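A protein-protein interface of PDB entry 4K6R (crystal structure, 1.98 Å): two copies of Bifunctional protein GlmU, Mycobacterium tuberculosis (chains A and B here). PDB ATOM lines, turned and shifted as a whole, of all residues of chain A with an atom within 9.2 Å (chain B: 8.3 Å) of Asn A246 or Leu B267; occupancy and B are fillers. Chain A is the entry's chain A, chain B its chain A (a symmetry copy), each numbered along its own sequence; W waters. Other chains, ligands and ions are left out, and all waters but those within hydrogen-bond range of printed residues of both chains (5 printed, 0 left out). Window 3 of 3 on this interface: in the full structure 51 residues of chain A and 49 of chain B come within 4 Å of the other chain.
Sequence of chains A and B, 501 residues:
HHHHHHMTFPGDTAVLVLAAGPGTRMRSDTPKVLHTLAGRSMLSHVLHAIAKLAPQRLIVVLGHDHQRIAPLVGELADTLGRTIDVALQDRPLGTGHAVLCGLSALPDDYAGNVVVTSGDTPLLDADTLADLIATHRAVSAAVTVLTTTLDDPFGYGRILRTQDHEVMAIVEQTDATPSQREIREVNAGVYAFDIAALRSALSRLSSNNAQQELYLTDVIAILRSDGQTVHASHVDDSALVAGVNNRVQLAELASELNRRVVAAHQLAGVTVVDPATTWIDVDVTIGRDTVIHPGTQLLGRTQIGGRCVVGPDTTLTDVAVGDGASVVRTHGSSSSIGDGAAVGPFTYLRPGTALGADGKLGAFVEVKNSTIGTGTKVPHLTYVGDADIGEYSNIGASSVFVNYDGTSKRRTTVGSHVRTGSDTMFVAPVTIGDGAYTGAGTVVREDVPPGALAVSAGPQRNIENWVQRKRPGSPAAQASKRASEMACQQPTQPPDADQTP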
ATOM      1  N   GLY A  23      14.645  20.729 -23.786  1.00  0.00           N
ATOM      2  CA  GLY A  23      13.268  20.715 -23.228  1.00  0.00           C
ATOM      3  C   GLY A  23      12.998  21.775 -22.181  1.00  0.00           C
ATOM      4  O   GLY A  23      12.337  21.477 -21.148  1.00  0.00           O
ATOM      5  N   THR A  24      13.471  23.003 -22.428  1.00  0.00           N
ATOM      6  CA  THR A  24      13.329  24.123 -21.470  1.00  0.00           C
ATOM      7  C   THR A  24      11.847  24.388 -21.140  1.00  0.00           C
ATOM      8  O   THR A  24      11.507  24.751 -20.017  1.00  0.00           O
ATOM      9  CB  THR A  24      13.976  25.461 -22.058  1.00  0.00           C
ATOM     10  OG1 THR A  24      15.326  25.217 -22.411  1.00  0.00           O
ATOM     11  CG2 THR A  24      13.917  26.652 -21.097  1.00  0.00           C
ATOM     12  N   ARG A  25      10.987  24.210 -22.135  1.00  0.00           N
ATOM     13  CA  ARG A  25       9.511  24.353 -21.938  1.00  0.00           C
ATOM     14  C   ARG A  25       8.913  23.382 -20.905  1.00  0.00           C
ATOM     15  O   ARG A  25       7.851  23.667 -20.366  1.00  0.00           O
ATOM     16  CB  ARG A  25       8.745  24.263 -23.273  1.00  0.00           C
ATOM     17  CG  ARG A  25       8.928  25.582 -24.052  1.00  0.00           C
ATOM     18  CD  ARG A  25       8.395  25.397 -25.469  1.00  0.00           C
ATOM     19  NE  ARG A  25       9.219  24.378 -26.180  1.00  0.00           N
ATOM     20  CZ  ARG A  25       8.947  23.980 -27.448  1.00  0.00           C
ATOM     21  NH1 ARG A  25       7.833  24.418 -28.075  1.00  0.00           N
ATOM     22  NH2 ARG A  25       9.747  23.117 -28.099  1.00  0.00           N
ATOM     23  N   MET A  26       9.609  22.285 -20.600  1.00  0.00           N
ATOM     24  CA  MET A  26       9.200  21.391 -19.487  1.00  0.00           C
ATOM     25  C   MET A  26       9.420  22.010 -18.129  1.00  0.00           C
ATOM     26  O   MET A  26       8.751  21.608 -17.154  1.00  0.00           O
ATOM     27  CB  MET A  26       9.942  20.045 -19.467  1.00  0.00           C
ATOM     28  CG  MET A  26       9.863  19.282 -20.801  1.00  0.00           C
ATOM     29  SD  MET A  26       8.213  18.550 -21.105  1.00  0.00           S
ATOM     30  CE  MET A  26       8.175  17.316 -19.834  1.00  0.00           C
ATOM     31  N   ARG A  27      10.307  22.996 -18.052  1.00  0.00           N
ATOM     32  CA  ARG A  27      10.680  23.590 -16.722  1.00  0.00           C
ATOM     33  C   ARG A  27      11.028  22.549 -15.661  1.00  0.00           C
ATOM     34  O   ARG A  27      10.441  22.466 -14.573  1.00  0.00           O
ATOM     35  CB  ARG A  27       9.568  24.520 -16.184  1.00  0.00           C
ATOM     36  CG  ARG A  27       9.128  25.577 -17.146  1.00  0.00           C
ATOM     37  CD  ARG A  27      10.034  26.736 -17.011  1.00  0.00           C
ATOM     38  NE  ARG A  27       9.422  27.950 -17.564  1.00  0.00           N
ATOM     39  CZ  ARG A  27       9.649  28.414 -18.791  1.00  0.00           C
ATOM     40  NH1 ARG A  27      10.463  27.768 -19.632  1.00  0.00           N
ATOM     41  NH2 ARG A  27       9.041  29.532 -19.176  1.00  0.00           N
ATOM     42  N   SER A  28      12.025  21.730 -15.955  1.00  0.00           N
ATOM     43  CA  SER A  28      12.316  20.647 -15.082  1.00  0.00           C
ATOM     44  C   SER A  28      13.845  20.449 -14.967  1.00  0.00           C
ATOM     45  O   SER A  28      14.563  20.660 -15.961  1.00  0.00           O
ATOM     46  CB  SER A  28      11.769  19.364 -15.763  1.00  0.00           C
ATOM     47  OG  SER A  28      11.982  18.255 -14.915  1.00  0.00           O
ATOM     48  N   LYS A  32      14.007  15.954 -20.235  1.00  0.00           N
ATOM     49  CA  LYS A  32      12.668  15.796 -20.804  1.00  0.00           C
ATOM     50  C   LYS A  32      12.346  14.404 -21.280  1.00  0.00           C
ATOM     51  O   LYS A  32      11.231  13.901 -20.980  1.00  0.00           O
ATOM     52  CB  LYS A  32      12.511  16.762 -21.990  1.00  0.00           C
ATOM     53  CG  LYS A  32      11.210  16.575 -22.808  1.00  0.00           C
ATOM     54  CD  LYS A  32      11.133  17.744 -23.825  1.00  0.00           C
ATOM     55  CE  LYS A  32      10.318  17.380 -24.978  1.00  0.00           C
ATOM     56  NZ  LYS A  32      10.457  18.426 -26.109  1.00  0.00           N
ATOM     57  N   HIS A  35      11.024  11.984 -18.750  1.00  0.00           N
ATOM     58  CA  HIS A  35       9.681  12.042 -18.100  1.00  0.00           C
ATOM     59  C   HIS A  35       8.805  10.863 -18.533  1.00  0.00           C
ATOM     60  O   HIS A  35       8.888  10.430 -19.675  1.00  0.00           O
ATOM     61  CB  HIS A  35       8.988  13.362 -18.360  1.00  0.00           C
ATOM     62  CG  HIS A  35       9.632  14.499 -17.638  1.00  0.00           C
ATOM     63  ND1 HIS A  35       8.942  15.299 -16.754  1.00  0.00           N
ATOM     64  CD2 HIS A  35      10.912  14.970 -17.668  1.00  0.00           C
ATOM     65  CE1 HIS A  35       9.752  16.237 -16.278  1.00  0.00           C
ATOM     66  NE2 HIS A  35      10.967  16.045 -16.802  1.00  0.00           N
ATOM     67  N   MET A  42       9.408   8.590 -22.029  1.00  0.00           N
ATOM     68  CA  MET A  42       9.186   8.853 -23.439  1.00  0.00           C
ATOM     69  C   MET A  42      10.277   8.177 -24.293  1.00  0.00           C
ATOM     70  O   MET A  42       9.952   7.552 -25.320  1.00  0.00           O
ATOM     71  CB  MET A  42       9.205  10.361 -23.707  1.00  0.00           C
ATOM     72  CG  MET A  42       7.977  11.046 -23.078  1.00  0.00           C
ATOM     73  SD  MET A  42       7.539  12.568 -23.986  1.00  0.00           S
ATOM     74  CE  MET A  42       8.957  13.606 -23.640  1.00  0.00           C
ATOM     75  N   ASP A 120      10.426  12.741 -28.486  1.00  0.00           N
ATOM     76  CA  ASP A 120       9.250  13.269 -27.707  1.00  0.00           C
ATOM     77  C   ASP A 120       7.950  12.978 -28.414  1.00  0.00           C
ATOM     78  O   ASP A 120       6.936  13.704 -28.195  1.00  0.00           O
ATOM     79  CB  ASP A 120       9.365  14.777 -27.334  1.00  0.00           C
ATOM     80  CG  ASP A 120       9.486  15.722 -28.595  1.00  0.00           C
ATOM     81  OD1 ASP A 120       9.455  15.248 -29.736  1.00  0.00           O
ATOM     82  OD2 ASP A 120       9.535  16.971 -28.466  1.00  0.00           O
ATOM     83  N   PHE A 154      -1.141  24.221 -32.293  1.00  0.00           N
ATOM     84  CA  PHE A 154      -0.153  25.127 -31.711  1.00  0.00           C
ATOM     85  C   PHE A 154       1.204  24.418 -31.513  1.00  0.00           C
ATOM     86  O   PHE A 154       1.275  23.315 -30.871  1.00  0.00           O
ATOM     87  CB  PHE A 154      -0.556  25.658 -30.327  1.00  0.00           C
ATOM     88  CG  PHE A 154       0.413  26.694 -29.769  1.00  0.00           C
ATOM     89  CD1 PHE A 154       1.106  26.475 -28.586  1.00  0.00           C
ATOM     90  CD2 PHE A 154       0.603  27.916 -30.431  1.00  0.00           C
ATOM     91  CE1 PHE A 154       2.033  27.467 -28.065  1.00  0.00           C
ATOM     92  CE2 PHE A 154       1.490  28.879 -29.963  1.00  0.00           C
ATOM     93  CZ  PHE A 154       2.216  28.656 -28.740  1.00  0.00           C
ATOM     94  N   GLY A 155       2.260  25.101 -31.976  1.00  0.00           N
ATOM     95  CA  GLY A 155       3.634  24.622 -31.791  1.00  0.00           C
ATOM     96  C   GLY A 155       4.105  23.534 -32.769  1.00  0.00           C
ATOM     97  O   GLY A 155       5.311  23.162 -32.764  1.00  0.00           O
ATOM     98  N   GLY A 243       3.311  15.156 -30.477  1.00  0.00           N
ATOM     99  CA  GLY A 243       4.511  15.415 -29.691  1.00  0.00           C
ATOM    100  C   GLY A 243       4.263  16.029 -28.340  1.00  0.00           C
ATOM    101  O   GLY A 243       3.126  16.534 -28.056  1.00  0.00           O
ATOM    102  N   VAL A 244       5.338  16.042 -27.529  1.00  0.00           N
ATOM    103  CA  VAL A 244       5.298  16.562 -26.186  1.00  0.00           C
ATOM    104  C   VAL A 244       6.401  17.581 -26.039  1.00  0.00           C
ATOM    105  O   VAL A 244       7.616  17.205 -25.992  1.00  0.00           O
ATOM    106  CB  VAL A 244       5.496  15.428 -25.164  1.00  0.00           C
ATOM    107  CG1 VAL A 244       5.700  15.949 -23.670  1.00  0.00           C
ATOM    108  CG2 VAL A 244       4.324  14.390 -25.192  1.00  0.00           C
ATOM    109  N   ASN A 245       6.037  18.856 -25.899  1.00  0.00           N
ATOM    110  CA  ASN A 245       7.058  19.846 -25.601  1.00  0.00           C
ATOM    111  C   ASN A 245       6.925  20.491 -24.252  1.00  0.00           C
ATOM    112  O   ASN A 245       7.754  21.329 -23.870  1.00  0.00           O
ATOM    113  CB  ASN A 245       7.027  20.966 -26.666  1.00  0.00           C
ATOM    114  CG  ASN A 245       7.688  20.557 -27.993  1.00  0.00           C
ATOM    115  OD1 ASN A 245       8.499  19.606 -28.068  1.00  0.00           O
ATOM    116  ND2 ASN A 245       7.280  21.233 -29.064  1.00  0.00           N
ATOM    117  N   ASN A 246       5.838  20.185 -23.517  1.00  0.00           N
ATOM    118  CA  ASN A 246       5.679  20.809 -22.215  1.00  0.00           C
ATOM    119  C   ASN A 246       4.815  19.827 -21.381  1.00  0.00           C
ATOM    120  O   ASN A 246       4.332  18.794 -21.929  1.00  0.00           O
ATOM    121  CB  ASN A 246       5.024  22.231 -22.303  1.00  0.00           C
ATOM    122  CG  ASN A 246       3.657  22.233 -22.917  1.00  0.00           C
ATOM    123  OD1 ASN A 246       2.787  21.353 -22.614  1.00  0.00           O
ATOM    124  ND2 ASN A 246       3.408  23.239 -23.784  1.00  0.00           N
ATOM    125  N   ARG A 247       4.633  20.161 -20.108  1.00  0.00           N
ATOM    126  CA  ARG A 247       3.933  19.240 -19.159  1.00  0.00           C
ATOM    127  C   ARG A 247       2.455  19.109 -19.449  1.00  0.00           C
ATOM    128  O   ARG A 247       1.855  18.071 -19.077  1.00  0.00           O
ATOM    129  CB  ARG A 247       4.183  19.676 -17.694  1.00  0.00           C
ATOM    130  CG  ARG A 247       5.614  19.245 -17.285  1.00  0.00           C
ATOM    131  CD  ARG A 247       5.890  19.113 -15.751  1.00  0.00           C
ATOM    132  NE  ARG A 247       7.113  19.681 -15.415  1.00  0.00           N
ATOM    133  CZ  ARG A 247       8.017  19.334 -14.524  1.00  0.00           C
ATOM    134  NH1 ARG A 247       8.014  18.292 -13.668  1.00  0.00           N
ATOM    135  NH2 ARG A 247       8.974  20.197 -14.502  1.00  0.00           N
ATOM    136  N   VAL A 248       1.866  20.129 -20.097  1.00  0.00           N
ATOM    137  CA  VAL A 248       0.457  20.095 -20.471  1.00  0.00           C
ATOM    138  C   VAL A 248       0.289  18.986 -21.522  1.00  0.00           C
ATOM    139  O   VAL A 248      -0.638  18.110 -21.397  1.00  0.00           O
ATOM    140  CB  VAL A 248      -0.045  21.469 -21.033  1.00  0.00           C
ATOM    141  CG1 VAL A 248      -1.504  21.408 -21.481  1.00  0.00           C
ATOM    142  CG2 VAL A 248       0.123  22.554 -19.942  1.00  0.00           C
ATOM    143  N   GLN A 249       1.125  19.045 -22.576  1.00  0.00           N
ATOM    144  CA  GLN A 249       1.103  18.010 -23.635  1.00  0.00           C
ATOM    145  C   GLN A 249       1.415  16.627 -23.114  1.00  0.00           C
ATOM    146  O   GLN A 249       0.800  15.580 -23.552  1.00  0.00           O
ATOM    147  CB  GLN A 249       2.050  18.343 -24.802  1.00  0.00           C
ATOM    148  CG  GLN A 249       1.536  19.662 -25.520  1.00  0.00           C
ATOM    149  CD  GLN A 249       2.320  20.010 -26.777  1.00  0.00           C
ATOM    150  OE1 GLN A 249       3.519  19.763 -26.845  1.00  0.00           O
ATOM    151  NE2 GLN A 249       1.659  20.623 -27.752  1.00  0.00           N
ATOM    152  N   LEU A 250       2.373  16.579 -22.197  1.00  0.00           N
ATOM    153  CA  LEU A 250       2.738  15.255 -21.608  1.00  0.00           C
ATOM    154  C   LEU A 250       1.471  14.602 -20.962  1.00  0.00           C
ATOM    155  O   LEU A 250       1.161  13.398 -21.202  1.00  0.00           O
ATOM    156  CB  LEU A 250       3.817  15.426 -20.520  1.00  0.00           C
ATOM    157  CG  LEU A 250       4.264  14.135 -19.761  1.00  0.00           C
ATOM    158  CD1 LEU A 250       4.637  13.034 -20.677  1.00  0.00           C
ATOM    159  CD2 LEU A 250       5.460  14.437 -18.782  1.00  0.00           C
ATOM    160  N   ALA A 251       0.785  15.373 -20.115  1.00  0.00           N
ATOM    161  CA  ALA A 251      -0.390  14.825 -19.364  1.00  0.00           C
ATOM    162  C   ALA A 251      -1.481  14.499 -20.361  1.00  0.00           C
ATOM    163  O   ALA A 251      -2.218  13.530 -20.166  1.00  0.00           O
ATOM    164  CB  ALA A 251      -0.907  15.800 -18.323  1.00  0.00           C
ATOM    165  N   GLU A 252      -1.651  15.301 -21.409  1.00  0.00           N
ATOM    166  CA  GLU A 252      -2.696  14.937 -22.343  1.00  0.00           C
ATOM    167  C   GLU A 252      -2.423  13.641 -23.147  1.00  0.00           C
ATOM    168  O   GLU A 252      -3.324  12.787 -23.339  1.00  0.00           O
ATOM    169  CB  GLU A 252      -3.244  16.145 -23.149  1.00  0.00           C
ATOM    170  CG  GLU A 252      -2.444  16.600 -24.154  1.00  0.00           C
ATOM    171  CD  GLU A 252      -2.746  18.118 -24.537  1.00  0.00           C
ATOM    172  OE1 GLU A 252      -3.574  18.862 -23.933  1.00  0.00           O
ATOM    173  OE2 GLU A 252      -2.083  18.566 -25.466  1.00  0.00           O
ATOM    174  N   LEU A 253      -1.174  13.398 -23.501  1.00  0.00           N
ATOM    175  CA  LEU A 253      -0.835  12.139 -24.167  1.00  0.00           C
ATOM    176  C   LEU A 253      -0.836  10.986 -23.207  1.00  0.00           C
ATOM    177  O   LEU A 253      -1.195   9.870 -23.628  1.00  0.00           O
ATOM    178  CB  LEU A 253       0.559  12.200 -24.855  1.00  0.00           C
ATOM    179  CG  LEU A 253       0.587  12.913 -26.220  1.00  0.00           C
ATOM    180  CD1 LEU A 253       1.885  12.430 -26.856  1.00  0.00           C
ATOM    181  CD2 LEU A 253      -0.674  12.501 -27.153  1.00  0.00           C
ATOM    182  N   ALA A 254      -0.477  11.223 -21.948  1.00  0.00           N
ATOM    183  CA  ALA A 254      -0.516  10.200 -20.933  1.00  0.00           C
ATOM    184  C   ALA A 254      -1.987   9.756 -20.745  1.00  0.00           C
ATOM    185  O   ALA A 254      -2.275   8.578 -20.565  1.00  0.00           O
ATOM    186  CB  ALA A 254       0.014  10.744 -19.641  1.00  0.00           C
ATOM    187  N   ARG B 260      -7.416  25.397 -16.187  1.00  0.00           N
ATOM    188  CA  ARG B 260      -6.506  26.507 -16.433  1.00  0.00           C
ATOM    189  C   ARG B 260      -5.554  26.744 -15.294  1.00  0.00           C
ATOM    190  O   ARG B 260      -4.372  27.078 -15.523  1.00  0.00           O
ATOM    191  CB  ARG B 260      -7.302  27.811 -16.648  1.00  0.00           C
ATOM    192  CG  ARG B 260      -8.138  27.717 -17.917  1.00  0.00           C
ATOM    193  CD  ARG B 260      -9.093  28.921 -18.149  1.00  0.00           C
ATOM    194  NE  ARG B 260      -9.816  28.598 -19.406  1.00  0.00           N
ATOM    195  CZ  ARG B 260     -10.103  29.478 -20.353  1.00  0.00           C
ATOM    196  NH1 ARG B 260      -9.745  30.758 -20.223  1.00  0.00           N
ATOM    197  NH2 ARG B 260     -10.740  29.063 -21.435  1.00  0.00           N
ATOM    198  N   VAL B 261      -6.027  26.614 -14.072  1.00  0.00           N
ATOM    199  CA  VAL B 261      -5.108  26.745 -12.914  1.00  0.00           C
ATOM    200  C   VAL B 261      -4.014  25.622 -13.006  1.00  0.00           C
ATOM    201  O   VAL B 261      -2.779  25.860 -12.842  1.00  0.00           O
ATOM    202  CB  VAL B 261      -5.868  26.598 -11.636  1.00  0.00           C
ATOM    203  CG1 VAL B 261      -4.955  26.421 -10.354  1.00  0.00           C
ATOM    204  CG2 VAL B 261      -6.767  27.847 -11.416  1.00  0.00           C
ATOM    205  N   VAL B 262      -4.480  24.392 -13.225  1.00  0.00           N
ATOM    206  CA  VAL B 262      -3.553  23.268 -13.342  1.00  0.00           C
ATOM    207  C   VAL B 262      -2.565  23.524 -14.470  1.00  0.00           C
ATOM    208  O   VAL B 262      -1.377  23.295 -14.284  1.00  0.00           O
ATOM    209  CB  VAL B 262      -4.334  21.941 -13.602  1.00  0.00           C
ATOM    210  CG1 VAL B 262      -3.390  20.845 -13.961  1.00  0.00           C
ATOM    211  CG2 VAL B 262      -5.046  21.550 -12.307  1.00  0.00           C
ATOM    212  N   ALA B 263      -3.055  23.967 -15.631  1.00  0.00           N
ATOM    213  CA  ALA B 263      -2.195  24.247 -16.800  1.00  0.00           C
ATOM    214  C   ALA B 263      -1.134  25.279 -16.458  1.00  0.00           C
ATOM    215  O   ALA B 263       0.035  25.088 -16.825  1.00  0.00           O
ATOM    216  CB  ALA B 263      -3.021  24.647 -18.065  1.00  0.00           C
ATOM    217  N   ALA B 264      -1.466  26.317 -15.688  1.00  0.00           N
ATOM    218  CA  ALA B 264      -0.468  27.329 -15.325  1.00  0.00           C
ATOM    219  C   ALA B 264       0.617  26.692 -14.471  1.00  0.00           C
ATOM    220  O   ALA B 264       1.814  26.929 -14.731  1.00  0.00           O
ATOM    221  CB  ALA B 264      -1.162  28.583 -14.591  1.00  0.00           C
ATOM    222  N   HIS B 265       0.265  25.779 -13.524  1.00  0.00           N
ATOM    223  CA  HIS B 265       1.281  25.082 -12.751  1.00  0.00           C
ATOM    224  C   HIS B 265       2.116  24.130 -13.630  1.00  0.00           C
ATOM    225  O   HIS B 265       3.356  24.060 -13.472  1.00  0.00           O
ATOM    226  CB  HIS B 265       0.681  24.297 -11.548  1.00  0.00           C
ATOM    227  CG  HIS B 265       0.112  25.199 -10.491  1.00  0.00           C
ATOM    228  ND1 HIS B 265       0.910  25.964  -9.657  1.00  0.00           N
ATOM    229  CD2 HIS B 265      -1.175  25.462 -10.138  1.00  0.00           C
ATOM    230  CE1 HIS B 265       0.129  26.693  -8.864  1.00  0.00           C
ATOM    231  NE2 HIS B 265      -1.138  26.374  -9.107  1.00  0.00           N
ATOM    232  N   GLN B 266       1.475  23.377 -14.531  1.00  0.00           N
ATOM    233  CA  GLN B 266       2.206  22.506 -15.411  1.00  0.00           C
ATOM    234  C   GLN B 266       3.245  23.287 -16.272  1.00  0.00           C
ATOM    235  O   GLN B 266       4.426  22.871 -16.382  1.00  0.00           O
ATOM    236  CB  GLN B 266       1.245  21.807 -16.374  1.00  0.00           C
ATOM    237  CG  GLN B 266       0.343  20.781 -15.647  1.00  0.00           C
ATOM    238  CD  GLN B 266      -0.700  20.282 -16.614  1.00  0.00           C
ATOM    239  OE1 GLN B 266      -1.442  21.072 -17.172  1.00  0.00           O
ATOM    240  NE2 GLN B 266      -0.740  18.974 -16.850  1.00  0.00           N
ATOM    241  N   LEU B 267       2.806  24.429 -16.826  1.00  0.00           N
ATOM    242  CA  LEU B 267       3.731  25.328 -17.618  1.00  0.00           C
ATOM    243  C   LEU B 267       4.835  25.902 -16.747  1.00  0.00           C
ATOM    244  O   LEU B 267       5.982  26.145 -17.226  1.00  0.00           O
ATOM    245  CB  LEU B 267       2.977  26.429 -18.397  1.00  0.00           C
ATOM    246  CG  LEU B 267       2.047  25.754 -19.438  1.00  0.00           C
ATOM    247  CD1 LEU B 267       1.175  26.780 -20.105  1.00  0.00           C
ATOM    248  CD2 LEU B 267       2.837  24.886 -20.528  1.00  0.00           C
ATOM    249  N   ALA B 268       4.556  26.077 -15.454  1.00  0.00           N
ATOM    250  CA  ALA B 268       5.590  26.589 -14.554  1.00  0.00           C
ATOM    251  C   ALA B 268       6.535  25.478 -14.037  1.00  0.00           C
ATOM    252  O   ALA B 268       7.469  25.790 -13.302  1.00  0.00           O
ATOM    253  CB  ALA B 268       4.986  27.396 -13.336  1.00  0.00           C
ATOM    254  N   GLY B 269       6.306  24.200 -14.340  1.00  0.00           N
ATOM    255  CA  GLY B 269       7.230  23.150 -13.917  1.00  0.00           C
ATOM    256  C   GLY B 269       6.663  22.123 -12.922  1.00  0.00           C
ATOM    257  O   GLY B 269       7.429  21.448 -12.210  1.00  0.00           O
ATOM    258  N   VAL B 270       5.330  21.991 -12.859  1.00  0.00           N
ATOM    259  CA  VAL B 270       4.711  21.019 -11.875  1.00  0.00           C
ATOM    260  C   VAL B 270       4.149  19.891 -12.744  1.00  0.00           C
ATOM    261  O   VAL B 270       3.401  20.130 -13.693  1.00  0.00           O
ATOM    262  CB  VAL B 270       3.540  21.626 -11.067  1.00  0.00           C
ATOM    263  CG1 VAL B 270       2.883  20.589 -10.076  1.00  0.00           C
ATOM    264  CG2 VAL B 270       4.032  22.914 -10.296  1.00  0.00           C
ATOM    265  N   THR B 271       4.567  18.692 -12.458  1.00  0.00           N
ATOM    266  CA  THR B 271       3.927  17.507 -13.041  1.00  0.00           C
ATOM    267  C   THR B 271       2.608  17.260 -12.318  1.00  0.00           C
ATOM    268  O   THR B 271       2.590  16.928 -11.127  1.00  0.00           O
ATOM    269  CB  THR B 271       4.826  16.240 -12.873  1.00  0.00           C
ATOM    270  OG1 THR B 271       5.964  16.440 -13.725  1.00  0.00           O
ATOM    271  CG2 THR B 271       4.108  14.952 -13.410  1.00  0.00           C
ATOM    272  N   VAL B 272       1.522  17.380 -13.070  1.00  0.00           N
ATOM    273  CA  VAL B 272       0.194  16.951 -12.587  1.00  0.00           C
ATOM    274  C   VAL B 272      -0.178  15.767 -13.455  1.00  0.00           C
ATOM    275  O   VAL B 272      -0.483  15.929 -14.630  1.00  0.00           O
ATOM    276  CB  VAL B 272      -0.844  18.099 -12.714  1.00  0.00           C
ATOM    277  CG1 VAL B 272      -2.250  17.625 -12.168  1.00  0.00           C
ATOM    278  CG2 VAL B 272      -0.388  19.299 -11.859  1.00  0.00           C
ATOM    279  N   ARG B 288       8.717  23.918  -8.284  1.00  0.00           N
ATOM    280  CA  ARG B 288       9.164  23.221  -9.453  1.00  0.00           C
ATOM    281  C   ARG B 288       9.508  21.742  -9.203  1.00  0.00           C
ATOM    282  O   ARG B 288      10.127  21.392  -8.176  1.00  0.00           O
ATOM    283  CB  ARG B 288      10.447  23.980  -9.942  1.00  0.00           C
ATOM    284  CG  ARG B 288      11.139  23.355 -11.144  1.00  0.00           C
ATOM    285  CD  ARG B 288      12.423  24.231 -11.362  1.00  0.00           C
ATOM    286  NE  ARG B 288      13.392  23.639 -12.251  1.00  0.00           N
ATOM    287  CZ  ARG B 288      13.485  24.006 -13.527  1.00  0.00           C
ATOM    288  NH1 ARG B 288      12.686  24.965 -14.019  1.00  0.00           N
ATOM    289  NH2 ARG B 288      14.408  23.485 -14.302  1.00  0.00           N
HETATM  290  O   HOH W   1      -2.624  18.355 -19.630  1.00  0.00           O
HETATM  291  O   HOH W   2       1.585  17.449 -15.942  1.00  0.00           O
HETATM  292  O   HOH W   3       6.688  25.925 -20.136  1.00  0.00           O
HETATM  293  O   HOH W   4       6.667  14.504 -15.405  1.00  0.00           O
HETATM  294  O   HOH W   5       5.736  22.447 -18.802  1.00  0.00           O
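The backbone carbonyl oxygen of Arg A27 lies close to the guanidinium group of Arg B288.
The backbone carbonyl oxygen (O) of Ser A28 sits close to the guanidinium group (NH2) of Arg B288.
The backbone carbonyl oxygen of Gly B269 lies within hydrogen-bond range of the guanidinium group of Arg A247.
The side-chain hydroxyl of Thr B271 lies within hydrogen-bond range of the guanidinium group of Arg A247 (2.8 Å).
The side-chain sulfur (SD) of Met A26 lies close to the backbone NH (N) of Asn A246 (3.8 Å).
O of Met A26 lies within hydrogen-bond range of NH2 of Arg A247, at 3.0 Å.
OD1 of Asn A246 lies within hydrogen-bond range of N of Val A248 (2.9 Å).
The side-chain amide oxygen of Asn A246 sits at hydrogen-bond distance from the backbone NH of Gln A249, 2.8 Å away.
Among the printed residues, pairs that only touch across the chains: Arg A27 with Leu B267, Arg A27 with Gly B269, Arg A247 with Val B270, Arg A247 with Gln B266, Ala A251 with Gln B266, Val A248 with Gln B266, Val A248 with Leu B267, Asn A246 with Leu B267, Ala A251 with Val B272, Arg A27 with Ala B268 and Met A26 with Gly B269.
Of the printed residues of chain B, Met A26 touches Gly B269.
Asn A246 touches one residue of chain B.
Printed residues of chain B within 4 Å of Arg A247: Gln B266, Gly B269, Val B270 and Thr B271.
Printed residues of chain A within 4 Å of Gln B266: Arg A247 (3.5 Å), Val A248 (3.5 Å) and Ala A251 (3.5 Å).
Of chain A, only Arg A27, Asn A246 and Val A248 come within 4 Å of Leu B267.
Of chain A, only Arg A27 (3.8 Å) comes within 4 Å of Ala B268.
Of the printed residues of chain A, Thr B271 touches Arg A247 (2.8 Å).
Printed residues of chain A within 4 Å of Val B272: Ala A251 (3.7 Å).
The nearest residue of chain B that does not touch Asn A246 is Gln B266 (5.9 Å).
The nearest residue of chain A that does not touch Leu B267 is Arg A25 (4.4 Å).
The nearest printed residue of chain A that does not touch Thr B271 is His A35 (4.4 Å).
Of the 14 printed residues of chain B, 8 touch a printed residue of chain A.
Printed residues of chain B that touch a printed residue of chain A: Gln B266, Leu B267, Ala B268, Gly B269, Val B270, Thr B271, Val B272 and Arg B288.
Hydrophobic or aromatic side chains of chain B within 4 Å of the printed part of chain A: Leu B267.
Printed residues of chain A that touch a printed residue of chain B: Met A26, Arg A27, Ser A28, Asn A246, Arg A247, Val A248 and Ala A251.
Hydrophobic or aromatic side chains of chain A that line the printed part of chain B: Val A248 and Ala A251.
Among the printed residues, no Asp or Glu carboxylate lies within 4 Å of a Lys or Arg side-chain nitrogen of the other chain.
No position is printed for both chains.
Of the 15 pairs that touch across the chains among the printed residues, none has its exchanged pair printed and touching as well.
Water W3 bridges the backbone carbonyl oxygen (O) of Arg A25 (2.6 Å) and the backbone carbonyl oxygen (O) of Leu B267 (3.0 Å).
Water W4 lies within hydrogen-bond range of the side-chain hydroxyl (OG1) of Thr B271 (2.7 Å) and a ring nitrogen (ND1) of His A35 (2.8 Å).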
